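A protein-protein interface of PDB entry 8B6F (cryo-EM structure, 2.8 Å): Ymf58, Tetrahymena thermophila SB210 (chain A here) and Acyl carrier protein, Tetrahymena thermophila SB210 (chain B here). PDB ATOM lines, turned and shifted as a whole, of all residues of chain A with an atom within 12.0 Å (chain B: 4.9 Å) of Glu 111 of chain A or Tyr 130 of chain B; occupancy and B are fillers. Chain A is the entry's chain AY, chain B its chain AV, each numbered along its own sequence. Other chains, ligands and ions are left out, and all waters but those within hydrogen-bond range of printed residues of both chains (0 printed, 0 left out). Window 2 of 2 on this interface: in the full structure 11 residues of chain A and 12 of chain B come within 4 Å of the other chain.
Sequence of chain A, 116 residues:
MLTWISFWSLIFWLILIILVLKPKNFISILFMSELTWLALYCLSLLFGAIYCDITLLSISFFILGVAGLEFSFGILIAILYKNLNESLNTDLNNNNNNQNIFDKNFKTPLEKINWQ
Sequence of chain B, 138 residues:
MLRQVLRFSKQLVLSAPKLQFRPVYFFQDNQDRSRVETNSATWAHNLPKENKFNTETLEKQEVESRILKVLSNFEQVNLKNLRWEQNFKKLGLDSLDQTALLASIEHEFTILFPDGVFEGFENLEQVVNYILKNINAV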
ATOM      1  N   PHE A 106      17.142 -11.322 -33.546  1.00  0.00           N
ATOM      2  CA  PHE A 106      17.161 -10.217 -34.495  1.00  0.00           C
ATOM      3  C   PHE A 106      17.158  -8.895 -33.745  1.00  0.00           C
ATOM      4  O   PHE A 106      16.473  -8.745 -32.730  1.00  0.00           O
ATOM      5  CB  PHE A 106      15.958 -10.271 -35.446  1.00  0.00           C
ATOM      6  CG  PHE A 106      15.987 -11.428 -36.404  1.00  0.00           C
ATOM      7  CD1 PHE A 106      17.175 -11.848 -36.979  1.00  0.00           C
ATOM      8  CD2 PHE A 106      14.819 -12.093 -36.734  1.00  0.00           C
ATOM      9  CE1 PHE A 106      17.196 -12.910 -37.861  1.00  0.00           C
ATOM     10  CE2 PHE A 106      14.835 -13.154 -37.614  1.00  0.00           C
ATOM     11  CZ  PHE A 106      16.025 -13.563 -38.177  1.00  0.00           C
ATOM     12  N   LYS A 107      17.928  -7.939 -34.257  1.00  0.00           N
ATOM     13  CA  LYS A 107      17.995  -6.592 -33.712  1.00  0.00           C
ATOM     14  C   LYS A 107      17.692  -5.597 -34.819  1.00  0.00           C
ATOM     15  O   LYS A 107      17.855  -5.888 -36.006  1.00  0.00           O
ATOM     16  CB  LYS A 107      19.377  -6.284 -33.116  1.00  0.00           C
ATOM     17  CG  LYS A 107      19.758  -7.130 -31.918  1.00  0.00           C
ATOM     18  CD  LYS A 107      21.197  -6.869 -31.501  1.00  0.00           C
ATOM     19  CE  LYS A 107      21.548  -7.591 -30.209  1.00  0.00           C
ATOM     20  NZ  LYS A 107      21.207  -9.039 -30.253  1.00  0.00           N
ATOM     21  N   THR A 108      17.245  -4.414 -34.421  1.00  0.00           N
ATOM     22  CA  THR A 108      17.075  -3.343 -35.386  1.00  0.00           C
ATOM     23  C   THR A 108      18.438  -2.967 -35.963  1.00  0.00           C
ATOM     24  O   THR A 108      19.441  -2.981 -35.240  1.00  0.00           O
ATOM     25  CB  THR A 108      16.430  -2.121 -34.734  1.00  0.00           C
ATOM     26  OG1 THR A 108      16.285  -1.077 -35.704  1.00  0.00           O
ATOM     27  CG2 THR A 108      17.285  -1.615 -33.584  1.00  0.00           C
ATOM     28  N   PRO A 109      18.521  -2.630 -37.247  1.00  0.00           N
ATOM     29  CA  PRO A 109      19.829  -2.293 -37.819  1.00  0.00           C
ATOM     30  C   PRO A 109      20.329  -0.936 -37.351  1.00  0.00           C
ATOM     31  O   PRO A 109      20.402   0.017 -38.133  1.00  0.00           O
ATOM     32  CB  PRO A 109      19.565  -2.318 -39.330  1.00  0.00           C
ATOM     33  CG  PRO A 109      18.136  -1.977 -39.457  1.00  0.00           C
ATOM     34  CD  PRO A 109      17.448  -2.557 -38.252  1.00  0.00           C
ATOM     35  N   LEU A 110      20.672  -0.841 -36.069  1.00  0.00           N
ATOM     36  CA  LEU A 110      21.199   0.376 -35.472  1.00  0.00           C
ATOM     37  C   LEU A 110      22.421   0.038 -34.634  1.00  0.00           C
ATOM     38  O   LEU A 110      22.694  -1.127 -34.334  1.00  0.00           O
ATOM     39  CB  LEU A 110      20.150   1.084 -34.606  1.00  0.00           C
ATOM     40  CG  LEU A 110      18.972   1.727 -35.338  1.00  0.00           C
ATOM     41  CD1 LEU A 110      18.007   2.331 -34.339  1.00  0.00           C
ATOM     42  CD2 LEU A 110      19.448   2.784 -36.321  1.00  0.00           C
ATOM     43  N   GLU A 111      23.160   1.077 -34.260  1.00  0.00           N
ATOM     44  CA  GLU A 111      24.351   0.941 -33.431  1.00  0.00           C
ATOM     45  C   GLU A 111      24.170   1.496 -32.029  1.00  0.00           C
ATOM     46  O   GLU A 111      24.716   0.937 -31.077  1.00  0.00           O
ATOM     47  CB  GLU A 111      25.539   1.639 -34.105  1.00  0.00           C
ATOM     48  CG  GLU A 111      26.846   1.527 -33.335  1.00  0.00           C
ATOM     49  CD  GLU A 111      27.097   2.710 -32.421  1.00  0.00           C
ATOM     50  OE1 GLU A 111      26.880   3.859 -32.860  1.00  0.00           O
ATOM     51  OE2 GLU A 111      27.508   2.492 -31.263  1.00  0.00           O
ATOM     52  N   LYS A 112      23.411   2.576 -31.875  1.00  0.00           N
ATOM     53  CA  LYS A 112      23.170   3.170 -30.568  1.00  0.00           C
ATOM     54  C   LYS A 112      21.759   3.734 -30.543  1.00  0.00           C
ATOM     55  O   LYS A 112      21.382   4.499 -31.434  1.00  0.00           O
ATOM     56  CB  LYS A 112      24.193   4.269 -30.262  1.00  0.00           C
ATOM     57  CG  LYS A 112      24.222   5.383 -31.294  1.00  0.00           C
ATOM     58  CD  LYS A 112      25.413   6.303 -31.094  1.00  0.00           C
ATOM     59  CE  LYS A 112      25.341   7.021 -29.762  1.00  0.00           C
ATOM     60  NZ  LYS A 112      26.410   8.050 -29.624  1.00  0.00           N
ATOM     61  N   ILE A 113      20.985   3.346 -29.530  1.00  0.00           N
ATOM     62  CA  ILE A 113      19.624   3.855 -29.407  1.00  0.00           C
ATOM     63  C   ILE A 113      19.619   5.243 -28.780  1.00  0.00           C
ATOM     64  O   ILE A 113      18.773   6.077 -29.121  1.00  0.00           O
ATOM     65  CB  ILE A 113      18.759   2.875 -28.594  1.00  0.00           C
ATOM     66  CG1 ILE A 113      18.775   1.478 -29.225  1.00  0.00           C
ATOM     67  CG2 ILE A 113      17.331   3.388 -28.478  1.00  0.00           C
ATOM     68  CD1 ILE A 113      18.259   1.422 -30.648  1.00  0.00           C
ATOM     69  N   ASN A 114      20.546   5.517 -27.867  1.00  0.00           N
ATOM     70  CA  ASN A 114      20.615   6.785 -27.156  1.00  0.00           C
ATOM     71  C   ASN A 114      21.872   7.532 -27.571  1.00  0.00           C
ATOM     72  O   ASN A 114      22.974   6.979 -27.516  1.00  0.00           O
ATOM     73  CB  ASN A 114      20.614   6.563 -25.642  1.00  0.00           C
ATOM     74  CG  ASN A 114      19.393   5.808 -25.166  1.00  0.00           C
ATOM     75  OD1 ASN A 114      18.600   5.322 -25.968  1.00  0.00           O
ATOM     76  ND2 ASN A 114      19.241   5.695 -23.853  1.00  0.00           N
ATOM     77  N   TRP A 115      21.702   8.786 -27.985  1.00  0.00           N
ATOM     78  CA  TRP A 115      22.818   9.631 -28.384  1.00  0.00           C
ATOM     79  C   TRP A 115      23.221  10.633 -27.316  1.00  0.00           C
ATOM     80  O   TRP A 115      24.412  10.929 -27.180  1.00  0.00           O
ATOM     81  CB  TRP A 115      22.471  10.387 -29.671  1.00  0.00           C
ATOM     82  CG  TRP A 115      22.310   9.494 -30.858  1.00  0.00           C
ATOM     83  CD1 TRP A 115      21.233   8.716 -31.157  1.00  0.00           C
ATOM     84  CD2 TRP A 115      23.260   9.287 -31.910  1.00  0.00           C
ATOM     85  NE1 TRP A 115      21.451   8.036 -32.329  1.00  0.00           N
ATOM     86  CE2 TRP A 115      22.689   8.369 -32.812  1.00  0.00           C
ATOM     87  CE3 TRP A 115      24.537   9.789 -32.175  1.00  0.00           C
ATOM     88  CZ2 TRP A 115      23.351   7.942 -33.959  1.00  0.00           C
ATOM     89  CZ3 TRP A 115      25.193   9.365 -33.315  1.00  0.00           C
ATOM     90  CH2 TRP A 115      24.600   8.449 -34.194  1.00  0.00           C
ATOM     91  N   GLN A 116      22.263  11.153 -26.559  1.00  0.00           N
ATOM     92  CA  GLN A 116      22.544  12.130 -25.517  1.00  0.00           C
ATOM     93  C   GLN A 116      22.057  11.612 -24.170  1.00  0.00           C
ATOM     94  O   GLN A 116      22.531  12.035 -23.116  1.00  0.00           O
ATOM     95  CB  GLN A 116      21.881  13.468 -25.853  1.00  0.00           C
ATOM     96  CG  GLN A 116      21.924  14.491 -24.728  1.00  0.00           C
ATOM     97  CD  GLN A 116      21.347  15.828 -25.144  1.00  0.00           C
ATOM     98  OE1 GLN A 116      21.233  16.126 -26.330  1.00  0.00           O
ATOM     99  NE2 GLN A 116      20.973  16.641 -24.161  1.00  0.00           N
ATOM    100  OXT GLN A 116      21.179  10.751 -24.103  1.00  0.00           O
ATOM    101  N   LEU B 112      33.052  -2.850 -34.567  1.00  0.00           N
ATOM    102  CA  LEU B 112      33.906  -2.156 -35.520  1.00  0.00           C
ATOM    103  C   LEU B 112      33.729  -0.659 -35.322  1.00  0.00           C
ATOM    104  O   LEU B 112      32.615  -0.144 -35.452  1.00  0.00           O
ATOM    105  CB  LEU B 112      33.560  -2.560 -36.955  1.00  0.00           C
ATOM    106  CG  LEU B 112      34.653  -2.389 -38.006  1.00  0.00           C
ATOM    107  CD1 LEU B 112      35.800  -3.357 -37.764  1.00  0.00           C
ATOM    108  CD2 LEU B 112      34.074  -2.582 -39.390  1.00  0.00           C
ATOM    109  N   PHE B 113      34.817   0.029 -34.999  1.00  0.00           N
ATOM    110  CA  PHE B 113      34.763   1.467 -34.768  1.00  0.00           C
ATOM    111  C   PHE B 113      34.822   2.211 -36.097  1.00  0.00           C
ATOM    112  O   PHE B 113      35.777   2.018 -36.857  1.00  0.00           O
ATOM    113  CB  PHE B 113      35.925   1.909 -33.886  1.00  0.00           C
ATOM    114  CG  PHE B 113      35.885   1.352 -32.491  1.00  0.00           C
ATOM    115  CD1 PHE B 113      34.699   1.301 -31.778  1.00  0.00           C
ATOM    116  CD2 PHE B 113      37.042   0.883 -31.891  1.00  0.00           C
ATOM    117  CE1 PHE B 113      34.669   0.791 -30.495  1.00  0.00           C
ATOM    118  CE2 PHE B 113      37.018   0.372 -30.609  1.00  0.00           C
ATOM    119  CZ  PHE B 113      35.830   0.326 -29.911  1.00  0.00           C
ATOM    120  N   PRO B 114      33.837   3.058 -36.421  1.00  0.00           N
ATOM    121  CA  PRO B 114      33.993   3.947 -37.580  1.00  0.00           C
ATOM    122  C   PRO B 114      35.318   4.689 -37.549  1.00  0.00           C
ATOM    123  O   PRO B 114      35.944   4.803 -36.491  1.00  0.00           O
ATOM    124  CB  PRO B 114      32.808   4.911 -37.450  1.00  0.00           C
ATOM    125  CG  PRO B 114      31.802   4.209 -36.603  1.00  0.00           C
ATOM    126  CD  PRO B 114      32.440   3.011 -35.954  1.00  0.00           C
ATOM    127  N   VAL B 117      35.396   7.880 -35.027  1.00  0.00           N
ATOM    128  CA  VAL B 117      35.495   7.566 -33.605  1.00  0.00           C
ATOM    129  C   VAL B 117      36.814   6.867 -33.299  1.00  0.00           C
ATOM    130  O   VAL B 117      37.448   7.135 -32.273  1.00  0.00           O
ATOM    131  CB  VAL B 117      34.284   6.725 -33.154  1.00  0.00           C
ATOM    132  CG1 VAL B 117      32.988   7.467 -33.435  1.00  0.00           C
ATOM    133  CG2 VAL B 117      34.279   5.366 -33.829  1.00  0.00           C
ATOM    134  N   PHE B 121      39.235   8.580 -30.395  1.00  0.00           N
ATOM    135  CA  PHE B 121      39.500   8.043 -29.067  1.00  0.00           C
ATOM    136  C   PHE B 121      40.832   8.564 -28.544  1.00  0.00           C
ATOM    137  O   PHE B 121      41.844   8.536 -29.250  1.00  0.00           O
ATOM    138  CB  PHE B 121      39.513   6.514 -29.100  1.00  0.00           C
ATOM    139  CG  PHE B 121      38.153   5.891 -29.255  1.00  0.00           C
ATOM    140  CD1 PHE B 121      37.046   6.423 -28.615  1.00  0.00           C
ATOM    141  CD2 PHE B 121      37.987   4.764 -30.038  1.00  0.00           C
ATOM    142  CE1 PHE B 121      35.803   5.844 -28.760  1.00  0.00           C
ATOM    143  CE2 PHE B 121      36.750   4.181 -30.184  1.00  0.00           C
ATOM    144  CZ  PHE B 121      35.655   4.722 -29.545  1.00  0.00           C
ATOM    145  N   GLN B 126      36.725   6.952 -22.895  1.00  0.00           N
ATOM    146  CA  GLN B 126      35.910   7.175 -24.082  1.00  0.00           C
ATOM    147  C   GLN B 126      35.531   5.855 -24.740  1.00  0.00           C
ATOM    148  O   GLN B 126      34.393   5.679 -25.186  1.00  0.00           O
ATOM    149  CB  GLN B 126      36.652   8.074 -25.069  1.00  0.00           C
ATOM    150  CG  GLN B 126      36.894   9.480 -24.550  1.00  0.00           C
ATOM    151  CD  GLN B 126      37.772  10.294 -25.472  1.00  0.00           C
ATOM    152  OE1 GLN B 126      38.140   9.844 -26.554  1.00  0.00           O
ATOM    153  NE2 GLN B 126      38.110  11.505 -25.049  1.00  0.00           N
ATOM    154  N   VAL B 127      36.475   4.915 -24.814  1.00  0.00           N
ATOM    155  CA  VAL B 127      36.176   3.606 -25.384  1.00  0.00           C
ATOM    156  C   VAL B 127      35.114   2.899 -24.552  1.00  0.00           C
ATOM    157  O   VAL B 127      34.189   2.282 -25.093  1.00  0.00           O
ATOM    158  CB  VAL B 127      37.460   2.763 -25.495  1.00  0.00           C
ATOM    159  CG1 VAL B 127      37.155   1.399 -26.092  1.00  0.00           C
ATOM    160  CG2 VAL B 127      38.502   3.486 -26.327  1.00  0.00           C
ATOM    161  N   VAL B 128      35.228   2.974 -23.226  1.00  0.00           N
ATOM    162  CA  VAL B 128      34.249   2.330 -22.353  1.00  0.00           C
ATOM    163  C   VAL B 128      32.864   2.921 -22.587  1.00  0.00           C
ATOM    164  O   VAL B 128      31.871   2.196 -22.707  1.00  0.00           O
ATOM    165  CB  VAL B 128      34.678   2.456 -20.880  1.00  0.00           C
ATOM    166  CG1 VAL B 128      33.566   1.991 -19.946  1.00  0.00           C
ATOM    167  CG2 VAL B 128      35.936   1.651 -20.625  1.00  0.00           C
ATOM    168  N   ASN B 129      32.778   4.250 -22.660  1.00  0.00           N
ATOM    169  CA  ASN B 129      31.486   4.891 -22.880  1.00  0.00           C
ATOM    170  C   ASN B 129      30.900   4.505 -24.231  1.00  0.00           C
ATOM    171  O   ASN B 129      29.699   4.235 -24.341  1.00  0.00           O
ATOM    172  CB  ASN B 129      31.627   6.408 -22.778  1.00  0.00           C
ATOM    173  CG  ASN B 129      32.084   6.860 -21.409  1.00  0.00           C
ATOM    174  OD1 ASN B 129      31.843   6.187 -20.408  1.00  0.00           O
ATOM    175  ND2 ASN B 129      32.745   8.010 -21.357  1.00  0.00           N
ATOM    176  N   TYR B 130      31.731   4.480 -25.275  1.00  0.00           N
ATOM    177  CA  TYR B 130      31.237   4.110 -26.596  1.00  0.00           C
ATOM    178  C   TYR B 130      30.718   2.678 -26.608  1.00  0.00           C
ATOM    179  O   TYR B 130      29.656   2.401 -27.175  1.00  0.00           O
ATOM    180  CB  TYR B 130      32.343   4.286 -27.636  1.00  0.00           C
ATOM    181  CG  TYR B 130      31.906   3.963 -29.044  1.00  0.00           C
ATOM    182  CD1 TYR B 130      32.004   2.672 -29.547  1.00  0.00           C
ATOM    183  CD2 TYR B 130      31.390   4.951 -29.870  1.00  0.00           C
ATOM    184  CE1 TYR B 130      31.602   2.375 -30.832  1.00  0.00           C
ATOM    185  CE2 TYR B 130      30.983   4.664 -31.156  1.00  0.00           C
ATOM    186  CZ  TYR B 130      31.093   3.376 -31.631  1.00  0.00           C
ATOM    187  OH  TYR B 130      30.689   3.092 -32.914  1.00  0.00           O
ATOM    188  N   ILE B 131      31.449   1.756 -25.983  1.00  0.00           N
ATOM    189  CA  ILE B 131      31.021   0.361 -25.958  1.00  0.00           C
ATOM    190  C   ILE B 131      29.746   0.208 -25.138  1.00  0.00           C
ATOM    191  O   ILE B 131      28.881  -0.615 -25.460  1.00  0.00           O
ATOM    192  CB  ILE B 131      32.155  -0.536 -25.428  1.00  0.00           C
ATOM    193  CG1 ILE B 131      33.336  -0.515 -26.402  1.00  0.00           C
ATOM    194  CG2 ILE B 131      31.661  -1.964 -25.220  1.00  0.00           C
ATOM    195  CD1 ILE B 131      34.578  -1.207 -25.886  1.00  0.00           C
ATOM    196  N   LEU B 132      29.610   0.985 -24.063  1.00  0.00           N
ATOM    197  CA  LEU B 132      28.378   0.944 -23.283  1.00  0.00           C
ATOM    198  C   LEU B 132      27.181   1.399 -24.111  1.00  0.00           C
ATOM    199  O   LEU B 132      26.112   0.781 -24.057  1.00  0.00           O
ATOM    200  CB  LEU B 132      28.524   1.811 -22.032  1.00  0.00           C
ATOM    201  CG  LEU B 132      29.396   1.248 -20.908  1.00  0.00           C
ATOM    202  CD1 LEU B 132      29.554   2.268 -19.799  1.00  0.00           C
ATOM    203  CD2 LEU B 132      28.811  -0.040 -20.362  1.00  0.00           C
ATOM    204  N   LYS B 133      27.338   2.477 -24.880  1.00  0.00           N
ATOM    205  CA  LYS B 133      26.243   2.940 -25.726  1.00  0.00           C
ATOM    206  C   LYS B 133      25.929   1.929 -26.823  1.00  0.00           C
ATOM    207  O   LYS B 133      24.761   1.724 -27.172  1.00  0.00           O
ATOM    208  CB  LYS B 133      26.587   4.301 -26.331  1.00  0.00           C
ATOM    209  CG  LYS B 133      26.530   5.449 -25.333  1.00  0.00           C
ATOM    210  CD  LYS B 133      26.790   6.795 -25.997  1.00  0.00           C
ATOM    211  CE  LYS B 133      28.218   6.897 -26.519  1.00  0.00           C
ATOM    212  NZ  LYS B 133      28.531   8.259 -27.040  1.00  0.00           N
ATOM    213  N   ASN B 134      26.957   1.293 -27.381  1.00  0.00           N
ATOM    214  CA  ASN B 134      26.752   0.327 -28.452  1.00  0.00           C
ATOM    215  C   ASN B 134      25.899  -0.838 -27.968  1.00  0.00           C
ATOM    216  O   ASN B 134      26.087  -1.350 -26.862  1.00  0.00           O
ATOM    217  CB  ASN B 134      28.101  -0.184 -28.957  1.00  0.00           C
ATOM    218  CG  ASN B 134      27.959  -1.300 -29.969  1.00  0.00           C
ATOM    219  OD1 ASN B 134      27.754  -2.456 -29.608  1.00  0.00           O
ATOM    220  ND2 ASN B 134      28.081  -0.960 -31.245  1.00  0.00           N
ATOM    221  N   ILE B 135      24.960  -1.265 -28.814  1.00  0.00           N
ATOM    222  CA  ILE B 135      24.085  -2.385 -28.485  1.00  0.00           C
ATOM    223  C   ILE B 135      24.536  -3.693 -29.127  1.00  0.00           C
ATOM    224  O   ILE B 135      24.109  -4.766 -28.675  1.00  0.00           O
ATOM    225  CB  ILE B 135      22.624  -2.086 -28.886  1.00  0.00           C
ATOM    226  CG1 ILE B 135      22.502  -1.945 -30.406  1.00  0.00           C
ATOM    227  CG2 ILE B 135      22.135  -0.830 -28.178  1.00  0.00           C
ATOM    228  CD1 ILE B 135      21.085  -1.732 -30.899  1.00  0.00           C
ATOM    229  N   ASN B 136      25.368  -3.640 -30.166  1.00  0.00           N
ATOM    230  CA  ASN B 136      25.798  -4.848 -30.856  1.00  0.00           C
ATOM    231  C   ASN B 136      26.970  -5.542 -30.178  1.00  0.00           C
ATOM    232  O   ASN B 136      27.311  -6.662 -30.571  1.00  0.00           O
ATOM    233  CB  ASN B 136      26.183  -4.517 -32.299  1.00  0.00           C
ATOM    234  CG  ASN B 136      25.074  -3.816 -33.052  1.00  0.00           C
ATOM    235  OD1 ASN B 136      24.116  -4.443 -33.495  1.00  0.00           O
ATOM    236  ND2 ASN B 136      25.205  -2.505 -33.206  1.00  0.00           N
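The side-chain amide nitrogen (ND2) of Asn 134 of chain B sits close to the side-chain carboxylate (OE2) of Glu 111 of chain A (3.5 Å). N of Ile 135 of chain B lies within hydrogen-bond range of O of Glu 111 of chain A (3.2 Å). The side-chain amide nitrogen (ND2) of Asn 136 of chain B sits at hydrogen-bond distance from the backbone carbonyl oxygen (O) of Leu 110 of chain A (3.1 Å). The side-chain amino group of Lys 112 of chain A lies close to the side-chain amino group of Lys 133 of chain B, at 3.3 Å.
The side-chain amide oxygen (OD1) of Asn 134 of chain B is in hydrogen-bond range of the backbone NH (N) of Asn 136 of chain B (2.7 Å).
Ile 135 of chain B touches Leu 110 of chain A (CD1 to O, 3.8 Å). Tyr 130 of chain B touches Glu 111 of chain A (OH to OE2, 3.6 Å). Glu 111 of chain A touches Lys 133 of chain B (O to O, 3.98 Å). Asn 136 of chain B touches Glu 111 of chain A.
Of the printed residues of chain B, Glu 111 of chain A touches Tyr 130, Lys 133, Asn 134, Ile 135 and Asn 136. No residue of chain A comes within 4 Å of Phe 113 of chain B. No residue of chain A comes within 4 Å of Val 117 of chain B. No residue of chain A comes within 4 Å of Asn 129 of chain B. No residue of chain A comes within 4 Å of Ile 131 of chain B. Of the printed residues of chain A, Ile 135 of chain B touches Leu 110 and Glu 111. Printed residues of chain B within 4 Å of Leu 110 of chain A: Ile 135 (3.8 Å) and Asn 136 (3.1 Å). Printed residues of chain A within 4 Å of Lys 133 of chain B: Glu 111 (3.98 Å) and Lys 112 (3.3 Å). Of the printed residues of chain A, Asn 136 of chain B touches Leu 110 and Glu 111. Printed residues of chain B within 4 Å of Lys 112 of chain A: Lys 133 (3.3 Å). Pro 109 of chain A touches none of the printed residues of chain B.
Printed residues of chain A that touch a printed residue of chain B: Leu 110, Glu 111 and Lys 112. Along chain A the printed residues that touch a printed residue of chain B span positions 110 to 112. Of the 16 printed residues of chain B, 5 touch a printed residue of chain A. Printed residues of chain B that touch a printed residue of chain A: Tyr 130, Lys 133, Asn 134, Ile 135 and Asn 136. Hydrophobic or aromatic side chains of chain B that line the printed part of chain A: Tyr 130 and Ile 135. Along chain B the printed residues that touch a printed residue of chain A span positions 130 to 136.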
